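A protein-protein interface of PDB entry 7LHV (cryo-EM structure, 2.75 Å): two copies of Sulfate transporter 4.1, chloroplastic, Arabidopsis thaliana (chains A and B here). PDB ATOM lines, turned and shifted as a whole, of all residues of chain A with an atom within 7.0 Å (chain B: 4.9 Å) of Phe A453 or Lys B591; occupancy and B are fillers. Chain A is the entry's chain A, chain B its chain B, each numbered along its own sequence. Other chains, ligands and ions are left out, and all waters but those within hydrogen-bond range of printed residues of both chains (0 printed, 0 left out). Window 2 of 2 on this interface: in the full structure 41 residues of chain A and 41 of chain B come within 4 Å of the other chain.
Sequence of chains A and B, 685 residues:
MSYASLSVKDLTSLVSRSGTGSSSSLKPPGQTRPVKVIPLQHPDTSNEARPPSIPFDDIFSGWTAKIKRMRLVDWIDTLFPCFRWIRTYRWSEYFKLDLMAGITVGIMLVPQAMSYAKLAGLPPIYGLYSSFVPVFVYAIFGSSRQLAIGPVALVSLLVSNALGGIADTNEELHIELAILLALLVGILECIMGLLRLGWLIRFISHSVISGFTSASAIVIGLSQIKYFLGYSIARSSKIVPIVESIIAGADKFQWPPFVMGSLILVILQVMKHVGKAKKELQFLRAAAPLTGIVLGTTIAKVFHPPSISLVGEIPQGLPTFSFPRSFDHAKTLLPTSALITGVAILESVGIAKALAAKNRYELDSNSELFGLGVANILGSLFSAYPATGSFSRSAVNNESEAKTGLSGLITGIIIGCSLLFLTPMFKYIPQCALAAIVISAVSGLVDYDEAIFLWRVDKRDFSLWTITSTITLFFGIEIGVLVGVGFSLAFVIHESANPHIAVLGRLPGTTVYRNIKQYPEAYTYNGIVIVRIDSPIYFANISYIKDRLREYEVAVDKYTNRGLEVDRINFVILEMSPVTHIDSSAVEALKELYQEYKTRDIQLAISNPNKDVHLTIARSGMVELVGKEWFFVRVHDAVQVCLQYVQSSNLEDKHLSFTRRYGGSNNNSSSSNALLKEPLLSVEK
No position is printed for both chains.
Of the 5 pairs that touch across the chains among the printed residues, none has its exchanged pair printed and touching as well.
Phe A453 touches just these residues of chain B: Glu B588 (3.8 Å) and Lys B591 (3.8 Å).
Printed residues of chain B within 4 Å of Val A457: Ser B620 (3.7 Å).
Lys B591 touches just one residue of chain A: Phe A453 (3.8 Å).
Of the printed residues of chain A, Ser B620 touches Val A457 (3.7 Å).
The nearest residue of chain A that does not touch Lys B591 is Arg A456 (5.2 Å).
The nearest printed residue of chain B that does not touch Asp A458 is Val B587 (7.2 Å).
Of the 12 printed residues of chain A, 4 touch a printed residue of chain B.
Printed residues of chain B that touch a printed residue of chain A: Ser B584, Glu B588, Lys B591 and Ser B620.
Among the printed residues, no Asp or Glu carboxylate lies within 4 Å of a Lys or Arg side-chain nitrogen of the other chain.
Glu B588 touches Phe A453 (CG to CE2, 3.8 Å).
Phe A453 touches Lys B591.
CD2 of Leu A454 touches OG of Ser B584, 3.2 Å away.
CG2 of Val A457 touches CA of Ser B620, 3.7 Å away.
Asp A458 touches Ser B584.
NZ of Lys B591 lies within salt-bridge range of OE2 of Glu B588.
The side-chain amino group (NZ) of Lys B591 lies within hydrogen-bond range of the backbone carbonyl oxygen (O) of Ser B620 (3.3 Å).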
ATOM      1  N   TYR A 448     -16.298  19.385   6.364  1.00  0.00           N
ATOM      2  CA  TYR A 448     -14.957  19.830   6.004  1.00  0.00           C
ATOM      3  C   TYR A 448     -13.898  19.387   7.005  1.00  0.00           C
ATOM      4  O   TYR A 448     -12.705  19.409   6.677  1.00  0.00           O
ATOM      5  CB  TYR A 448     -14.922  21.354   5.877  1.00  0.00           C
ATOM      6  CG  TYR A 448     -15.333  22.081   7.136  1.00  0.00           C
ATOM      7  CD1 TYR A 448     -16.672  22.299   7.431  1.00  0.00           C
ATOM      8  CD2 TYR A 448     -14.383  22.546   8.033  1.00  0.00           C
ATOM      9  CE1 TYR A 448     -17.052  22.957   8.581  1.00  0.00           C
ATOM     10  CE2 TYR A 448     -14.753  23.207   9.187  1.00  0.00           C
ATOM     11  CZ  TYR A 448     -16.090  23.409   9.455  1.00  0.00           C
ATOM     12  OH  TYR A 448     -16.463  24.067  10.602  1.00  0.00           O
ATOM     13  N   ASP A 449     -14.300  18.998   8.216  1.00  0.00           N
ATOM     14  CA  ASP A 449     -13.334  18.502   9.189  1.00  0.00           C
ATOM     15  C   ASP A 449     -12.649  17.240   8.684  1.00  0.00           C
ATOM     16  O   ASP A 449     -11.436  17.073   8.850  1.00  0.00           O
ATOM     17  CB  ASP A 449     -14.020  18.240  10.527  1.00  0.00           C
ATOM     18  CG  ASP A 449     -13.911  19.416  11.474  1.00  0.00           C
ATOM     19  OD1 ASP A 449     -13.181  20.375  11.150  1.00  0.00           O
ATOM     20  OD2 ASP A 449     -14.553  19.379  12.544  1.00  0.00           O
ATOM     21  N   GLU A 450     -13.411  16.342   8.055  1.00  0.00           N
ATOM     22  CA  GLU A 450     -12.797  15.159   7.466  1.00  0.00           C
ATOM     23  C   GLU A 450     -11.884  15.538   6.313  1.00  0.00           C
ATOM     24  O   GLU A 450     -10.863  14.886   6.090  1.00  0.00           O
ATOM     25  CB  GLU A 450     -13.863  14.178   6.991  1.00  0.00           C
ATOM     26  CG  GLU A 450     -13.329  12.807   6.631  1.00  0.00           C
ATOM     27  CD  GLU A 450     -12.804  12.058   7.840  1.00  0.00           C
ATOM     28  OE1 GLU A 450     -13.263  12.344   8.967  1.00  0.00           O
ATOM     29  OE2 GLU A 450     -11.933  11.179   7.669  1.00  0.00           O
ATOM     30  N   ALA A 451     -12.233  16.582   5.560  1.00  0.00           N
ATOM     31  CA  ALA A 451     -11.349  17.035   4.490  1.00  0.00           C
ATOM     32  C   ALA A 451     -10.015  17.511   5.048  1.00  0.00           C
ATOM     33  O   ALA A 451      -8.951  17.183   4.506  1.00  0.00           O
ATOM     34  CB  ALA A 451     -12.020  18.145   3.686  1.00  0.00           C
ATOM     35  N   ILE A 452     -10.050  18.276   6.139  1.00  0.00           N
ATOM     36  CA  ILE A 452      -8.812  18.728   6.771  1.00  0.00           C
ATOM     37  C   ILE A 452      -8.019  17.541   7.304  1.00  0.00           C
ATOM     38  O   ILE A 452      -6.792  17.474   7.154  1.00  0.00           O
ATOM     39  CB  ILE A 452      -9.125  19.751   7.875  1.00  0.00           C
ATOM     40  CG1 ILE A 452      -9.683  21.032   7.262  1.00  0.00           C
ATOM     41  CG2 ILE A 452      -7.884  20.053   8.691  1.00  0.00           C
ATOM     42  CD1 ILE A 452     -10.161  22.033   8.279  1.00  0.00           C
ATOM     43  N   PHE A 453      -8.707  16.584   7.931  1.00  0.00           N
ATOM     44  CA  PHE A 453      -8.027  15.401   8.452  1.00  0.00           C
ATOM     45  C   PHE A 453      -7.362  14.606   7.334  1.00  0.00           C
ATOM     46  O   PHE A 453      -6.220  14.153   7.478  1.00  0.00           O
ATOM     47  CB  PHE A 453      -9.022  14.528   9.211  1.00  0.00           C
ATOM     48  CG  PHE A 453      -8.425  13.280   9.781  1.00  0.00           C
ATOM     49  CD1 PHE A 453      -7.620  13.332  10.902  1.00  0.00           C
ATOM     50  CD2 PHE A 453      -8.676  12.051   9.197  1.00  0.00           C
ATOM     51  CE1 PHE A 453      -7.075  12.183  11.429  1.00  0.00           C
ATOM     52  CE2 PHE A 453      -8.132  10.899   9.720  1.00  0.00           C
ATOM     53  CZ  PHE A 453      -7.331  10.964  10.837  1.00  0.00           C
ATOM     54  N   LEU A 454      -8.063  14.426   6.213  1.00  0.00           N
ATOM     55  CA  LEU A 454      -7.489  13.714   5.078  1.00  0.00           C
ATOM     56  C   LEU A 454      -6.287  14.455   4.517  1.00  0.00           C
ATOM     57  O   LEU A 454      -5.273  13.837   4.179  1.00  0.00           O
ATOM     58  CB  LEU A 454      -8.544  13.515   3.990  1.00  0.00           C
ATOM     59  CG  LEU A 454      -9.732  12.628   4.349  1.00  0.00           C
ATOM     60  CD1 LEU A 454     -10.684  12.510   3.178  1.00  0.00           C
ATOM     61  CD2 LEU A 454      -9.258  11.270   4.799  1.00  0.00           C
ATOM     62  N   TRP A 455      -6.380  15.781   4.404  1.00  0.00           N
ATOM     63  CA  TRP A 455      -5.235  16.545   3.928  1.00  0.00           C
ATOM     64  C   TRP A 455      -4.043  16.360   4.856  1.00  0.00           C
ATOM     65  O   TRP A 455      -2.895  16.291   4.400  1.00  0.00           O
ATOM     66  CB  TRP A 455      -5.590  18.025   3.815  1.00  0.00           C
ATOM     67  CG  TRP A 455      -4.404  18.884   3.533  1.00  0.00           C
ATOM     68  CD1 TRP A 455      -3.636  19.549   4.441  1.00  0.00           C
ATOM     69  CD2 TRP A 455      -3.851  19.178   2.247  1.00  0.00           C
ATOM     70  NE1 TRP A 455      -2.634  20.234   3.800  1.00  0.00           N
ATOM     71  CE2 TRP A 455      -2.745  20.023   2.452  1.00  0.00           C
ATOM     72  CE3 TRP A 455      -4.184  18.807   0.942  1.00  0.00           C
ATOM     73  CZ2 TRP A 455      -1.971  20.503   1.401  1.00  0.00           C
ATOM     74  CZ3 TRP A 455      -3.415  19.283  -0.098  1.00  0.00           C
ATOM     75  CH2 TRP A 455      -2.322  20.122   0.136  1.00  0.00           C
ATOM     76  N   ARG A 456      -4.296  16.279   6.162  1.00  0.00           N
ATOM     77  CA  ARG A 456      -3.205  16.095   7.110  1.00  0.00           C
ATOM     78  C   ARG A 456      -2.602  14.698   7.010  1.00  0.00           C
ATOM     79  O   ARG A 456      -1.382  14.537   7.125  1.00  0.00           O
ATOM     80  CB  ARG A 456      -3.694  16.368   8.530  1.00  0.00           C
ATOM     81  CG  ARG A 456      -2.633  16.190   9.600  1.00  0.00           C
ATOM     82  CD  ARG A 456      -3.117  16.726  10.934  1.00  0.00           C
ATOM     83  NE  ARG A 456      -4.302  16.018  11.405  1.00  0.00           N
ATOM     84  CZ  ARG A 456      -4.418  15.473  12.609  1.00  0.00           C
ATOM     85  NH1 ARG A 456      -3.437  15.534  13.493  1.00  0.00           N
ATOM     86  NH2 ARG A 456      -5.550  14.853  12.931  1.00  0.00           N
ATOM     87  N   VAL A 457      -3.430  13.677   6.793  1.00  0.00           N
ATOM     88  CA  VAL A 457      -2.962  12.298   6.912  1.00  0.00           C
ATOM     89  C   VAL A 457      -2.721  11.655   5.550  1.00  0.00           C
ATOM     90  O   VAL A 457      -1.587  11.286   5.224  1.00  0.00           O
ATOM     91  CB  VAL A 457      -3.951  11.457   7.737  1.00  0.00           C
ATOM     92  CG1 VAL A 457      -3.590   9.987   7.656  1.00  0.00           C
ATOM     93  CG2 VAL A 457      -3.950  11.919   9.180  1.00  0.00           C
ATOM     94  N   ASP A 458      -3.774  11.509   4.747  1.00  0.00           N
ATOM     95  CA  ASP A 458      -3.718  10.723   3.518  1.00  0.00           C
ATOM     96  C   ASP A 458      -4.164  11.585   2.347  1.00  0.00           C
ATOM     97  O   ASP A 458      -5.358  11.861   2.198  1.00  0.00           O
ATOM     98  CB  ASP A 458      -4.590   9.473   3.632  1.00  0.00           C
ATOM     99  CG  ASP A 458      -4.258   8.434   2.584  1.00  0.00           C
ATOM    100  OD1 ASP A 458      -3.335   8.670   1.779  1.00  0.00           O
ATOM    101  OD2 ASP A 458      -4.926   7.382   2.559  1.00  0.00           O
ATOM    102  N   PHE A 462      -7.727  12.496   0.384  1.00  0.00           N
ATOM    103  CA  PHE A 462      -8.128  13.885   0.192  1.00  0.00           C
ATOM    104  C   PHE A 462      -8.439  14.169  -1.270  1.00  0.00           C
ATOM    105  O   PHE A 462      -9.390  14.893  -1.580  1.00  0.00           O
ATOM    106  CB  PHE A 462      -7.039  14.829   0.695  1.00  0.00           C
ATOM    107  CG  PHE A 462      -7.336  16.279   0.443  1.00  0.00           C
ATOM    108  CD1 PHE A 462      -8.146  16.989   1.309  1.00  0.00           C
ATOM    109  CD2 PHE A 462      -6.812  16.930  -0.658  1.00  0.00           C
ATOM    110  CE1 PHE A 462      -8.425  18.319   1.082  1.00  0.00           C
ATOM    111  CE2 PHE A 462      -7.091  18.260  -0.890  1.00  0.00           C
ATOM    112  CZ  PHE A 462      -7.897  18.953  -0.017  1.00  0.00           C
ATOM    113  N   SER B 584      -6.116   6.498   5.788  1.00  0.00           N
ATOM    114  CA  SER B 584      -6.820   7.272   6.807  1.00  0.00           C
ATOM    115  C   SER B 584      -7.923   6.457   7.471  1.00  0.00           C
ATOM    116  O   SER B 584      -8.139   6.562   8.685  1.00  0.00           O
ATOM    117  CB  SER B 584      -7.402   8.535   6.184  1.00  0.00           C
ATOM    118  OG  SER B 584      -8.521   8.215   5.379  1.00  0.00           O
ATOM    119  N   VAL B 587      -6.478   4.298  10.365  1.00  0.00           N
ATOM    120  CA  VAL B 587      -6.180   4.952  11.636  1.00  0.00           C
ATOM    121  C   VAL B 587      -7.458   5.425  12.317  1.00  0.00           C
ATOM    122  O   VAL B 587      -7.567   5.389  13.547  1.00  0.00           O
ATOM    123  CB  VAL B 587      -5.169   6.097  11.445  1.00  0.00           C
ATOM    124  CG1 VAL B 587      -3.784   5.533  11.198  1.00  0.00           C
ATOM    125  CG2 VAL B 587      -5.581   6.995  10.306  1.00  0.00           C
ATOM    126  N   GLU B 588      -8.449   5.873  11.538  1.00  0.00           N
ATOM    127  CA  GLU B 588      -9.728   6.244  12.140  1.00  0.00           C
ATOM    128  C   GLU B 588     -10.378   5.049  12.830  1.00  0.00           C
ATOM    129  O   GLU B 588     -10.848   5.152  13.972  1.00  0.00           O
ATOM    130  CB  GLU B 588     -10.661   6.832  11.084  1.00  0.00           C
ATOM    131  CG  GLU B 588     -10.617   8.347  11.006  1.00  0.00           C
ATOM    132  CD  GLU B 588     -11.186   9.008  12.251  1.00  0.00           C
ATOM    133  OE1 GLU B 588     -12.373   8.775  12.561  1.00  0.00           O
ATOM    134  OE2 GLU B 588     -10.445   9.758  12.922  1.00  0.00           O
ATOM    135  N   ALA B 589     -10.400   3.897  12.158  1.00  0.00           N
ATOM    136  CA  ALA B 589     -10.969   2.702  12.768  1.00  0.00           C
ATOM    137  C   ALA B 589     -10.155   2.257  13.974  1.00  0.00           C
ATOM    138  O   ALA B 589     -10.718   1.787  14.964  1.00  0.00           O
ATOM    139  CB  ALA B 589     -11.064   1.578  11.741  1.00  0.00           C
ATOM    140  N   LEU B 590      -8.830   2.383  13.906  1.00  0.00           N
ATOM    141  CA  LEU B 590      -8.003   2.004  15.044  1.00  0.00           C
ATOM    142  C   LEU B 590      -8.297   2.879  16.255  1.00  0.00           C
ATOM    143  O   LEU B 590      -8.377   2.383  17.383  1.00  0.00           O
ATOM    144  CB  LEU B 590      -6.525   2.078  14.664  1.00  0.00           C
ATOM    145  CG  LEU B 590      -5.991   0.890  13.861  1.00  0.00           C
ATOM    146  CD1 LEU B 590      -4.535   1.101  13.488  1.00  0.00           C
ATOM    147  CD2 LEU B 590      -6.164  -0.400  14.642  1.00  0.00           C
ATOM    148  N   LYS B 591      -8.478   4.184  16.037  1.00  0.00           N
ATOM    149  CA  LYS B 591      -8.845   5.069  17.138  1.00  0.00           C
ATOM    150  C   LYS B 591     -10.218   4.717  17.699  1.00  0.00           C
ATOM    151  O   LYS B 591     -10.420   4.723  18.922  1.00  0.00           O
ATOM    152  CB  LYS B 591      -8.805   6.525  16.677  1.00  0.00           C
ATOM    153  CG  LYS B 591      -7.400   7.061  16.468  1.00  0.00           C
ATOM    154  CD  LYS B 591      -7.386   8.574  16.359  1.00  0.00           C
ATOM    155  CE  LYS B 591      -7.871   9.040  14.999  1.00  0.00           C
ATOM    156  NZ  LYS B 591      -7.558  10.477  14.772  1.00  0.00           N
ATOM    157  N   GLU B 592     -11.176   4.405  16.822  1.00  0.00           N
ATOM    158  CA  GLU B 592     -12.504   4.021  17.296  1.00  0.00           C
ATOM    159  C   GLU B 592     -12.453   2.744  18.129  1.00  0.00           C
ATOM    160  O   GLU B 592     -13.089   2.659  19.188  1.00  0.00           O
ATOM    161  CB  GLU B 592     -13.460   3.854  16.117  1.00  0.00           C
ATOM    162  CG  GLU B 592     -13.785   5.149  15.400  1.00  0.00           C
ATOM    163  CD  GLU B 592     -14.682   4.937  14.197  1.00  0.00           C
ATOM    164  OE1 GLU B 592     -15.143   3.795  13.992  1.00  0.00           O
ATOM    165  OE2 GLU B 592     -14.926   5.913  13.457  1.00  0.00           O
ATOM    166  N   LEU B 593     -11.707   1.737  17.668  1.00  0.00           N
ATOM    167  CA  LEU B 593     -11.579   0.500  18.436  1.00  0.00           C
ATOM    168  C   LEU B 593     -10.840   0.726  19.745  1.00  0.00           C
ATOM    169  O   LEU B 593     -11.161   0.091  20.754  1.00  0.00           O
ATOM    170  CB  LEU B 593     -10.896  -0.592  17.611  1.00  0.00           C
ATOM    171  CG  LEU B 593     -11.732  -1.428  16.637  1.00  0.00           C
ATOM    172  CD1 LEU B 593     -12.752  -2.229  17.421  1.00  0.00           C
ATOM    173  CD2 LEU B 593     -12.441  -0.601  15.591  1.00  0.00           C
ATOM    174  N   TYR B 594      -9.847   1.617  19.763  1.00  0.00           N
ATOM    175  CA  TYR B 594      -9.184   1.920  21.026  1.00  0.00           C
ATOM    176  C   TYR B 594     -10.152   2.554  22.017  1.00  0.00           C
ATOM    177  O   TYR B 594     -10.150   2.216  23.207  1.00  0.00           O
ATOM    178  CB  TYR B 594      -7.990   2.839  20.802  1.00  0.00           C
ATOM    179  CG  TYR B 594      -7.460   3.404  22.094  1.00  0.00           C
ATOM    180  CD1 TYR B 594      -6.816   2.591  23.013  1.00  0.00           C
ATOM    181  CD2 TYR B 594      -7.628   4.742  22.411  1.00  0.00           C
ATOM    182  CE1 TYR B 594      -6.339   3.099  24.200  1.00  0.00           C
ATOM    183  CE2 TYR B 594      -7.155   5.259  23.597  1.00  0.00           C
ATOM    184  CZ  TYR B 594      -6.511   4.433  24.488  1.00  0.00           C
ATOM    185  OH  TYR B 594      -6.036   4.945  25.672  1.00  0.00           O
ATOM    186  N   GLN B 595     -10.984   3.486  21.545  1.00  0.00           N
ATOM    187  CA  GLN B 595     -11.967   4.101  22.430  1.00  0.00           C
ATOM    188  C   GLN B 595     -12.969   3.071  22.939  1.00  0.00           C
ATOM    189  O   GLN B 595     -13.313   3.060  24.127  1.00  0.00           O
ATOM    190  CB  GLN B 595     -12.680   5.243  21.709  1.00  0.00           C
ATOM    191  CG  GLN B 595     -11.797   6.456  21.466  1.00  0.00           C
ATOM    192  CD  GLN B 595     -12.466   7.501  20.599  1.00  0.00           C
ATOM    193  OE1 GLN B 595     -13.399   7.203  19.857  1.00  0.00           O
ATOM    194  NE2 GLN B 595     -11.988   8.735  20.689  1.00  0.00           N
ATOM    195  N   SER B 620      -1.586  10.750  12.264  1.00  0.00           N
ATOM    196  CA  SER B 620      -3.004  10.771  12.603  1.00  0.00           C
ATOM    197  C   SER B 620      -3.264  11.106  14.065  1.00  0.00           C
ATOM    198  O   SER B 620      -4.426  11.305  14.436  1.00  0.00           O
ATOM    199  CB  SER B 620      -3.650   9.427  12.268  1.00  0.00           C
ATOM    200  OG  SER B 620      -3.133   8.396  13.087  1.00  0.00           O
ATOM    201  N   MET B 622      -2.673   9.043  16.623  1.00  0.00           N
ATOM    202  CA  MET B 622      -3.010   7.859  17.404  1.00  0.00           C
ATOM    203  C   MET B 622      -1.996   7.598  18.509  1.00  0.00           C
ATOM    204  O   MET B 622      -2.365   7.086  19.574  1.00  0.00           O
ATOM    205  CB  MET B 622      -3.121   6.643  16.486  1.00  0.00           C
ATOM    206  CG  MET B 622      -3.546   5.377  17.198  1.00  0.00           C
ATOM    207  SD  MET B 622      -3.761   3.974  16.092  1.00  0.00           S
ATOM    208  CE  MET B 622      -4.141   2.686  17.276  1.00  0.00           C
ATOM    209  N   LEU B 625      -2.950   9.564  21.436  1.00  0.00           N
ATOM    210  CA  LEU B 625      -4.219   9.120  22.004  1.00  0.00           C
ATOM    211  C   LEU B 625      -4.043   7.861  22.844  1.00  0.00           C
ATOM    212  O   LEU B 625      -4.547   7.780  23.969  1.00  0.00           O
ATOM    213  CB  LEU B 625      -5.239   8.885  20.891  1.00  0.00           C
ATOM    214  CG  LEU B 625      -6.512   8.145  21.301  1.00  0.00           C
ATOM    215  CD1 LEU B 625      -7.456   9.076  22.035  1.00  0.00           C
ATOM    216  CD2 LEU B 625      -7.194   7.538  20.091  1.00  0.00           C
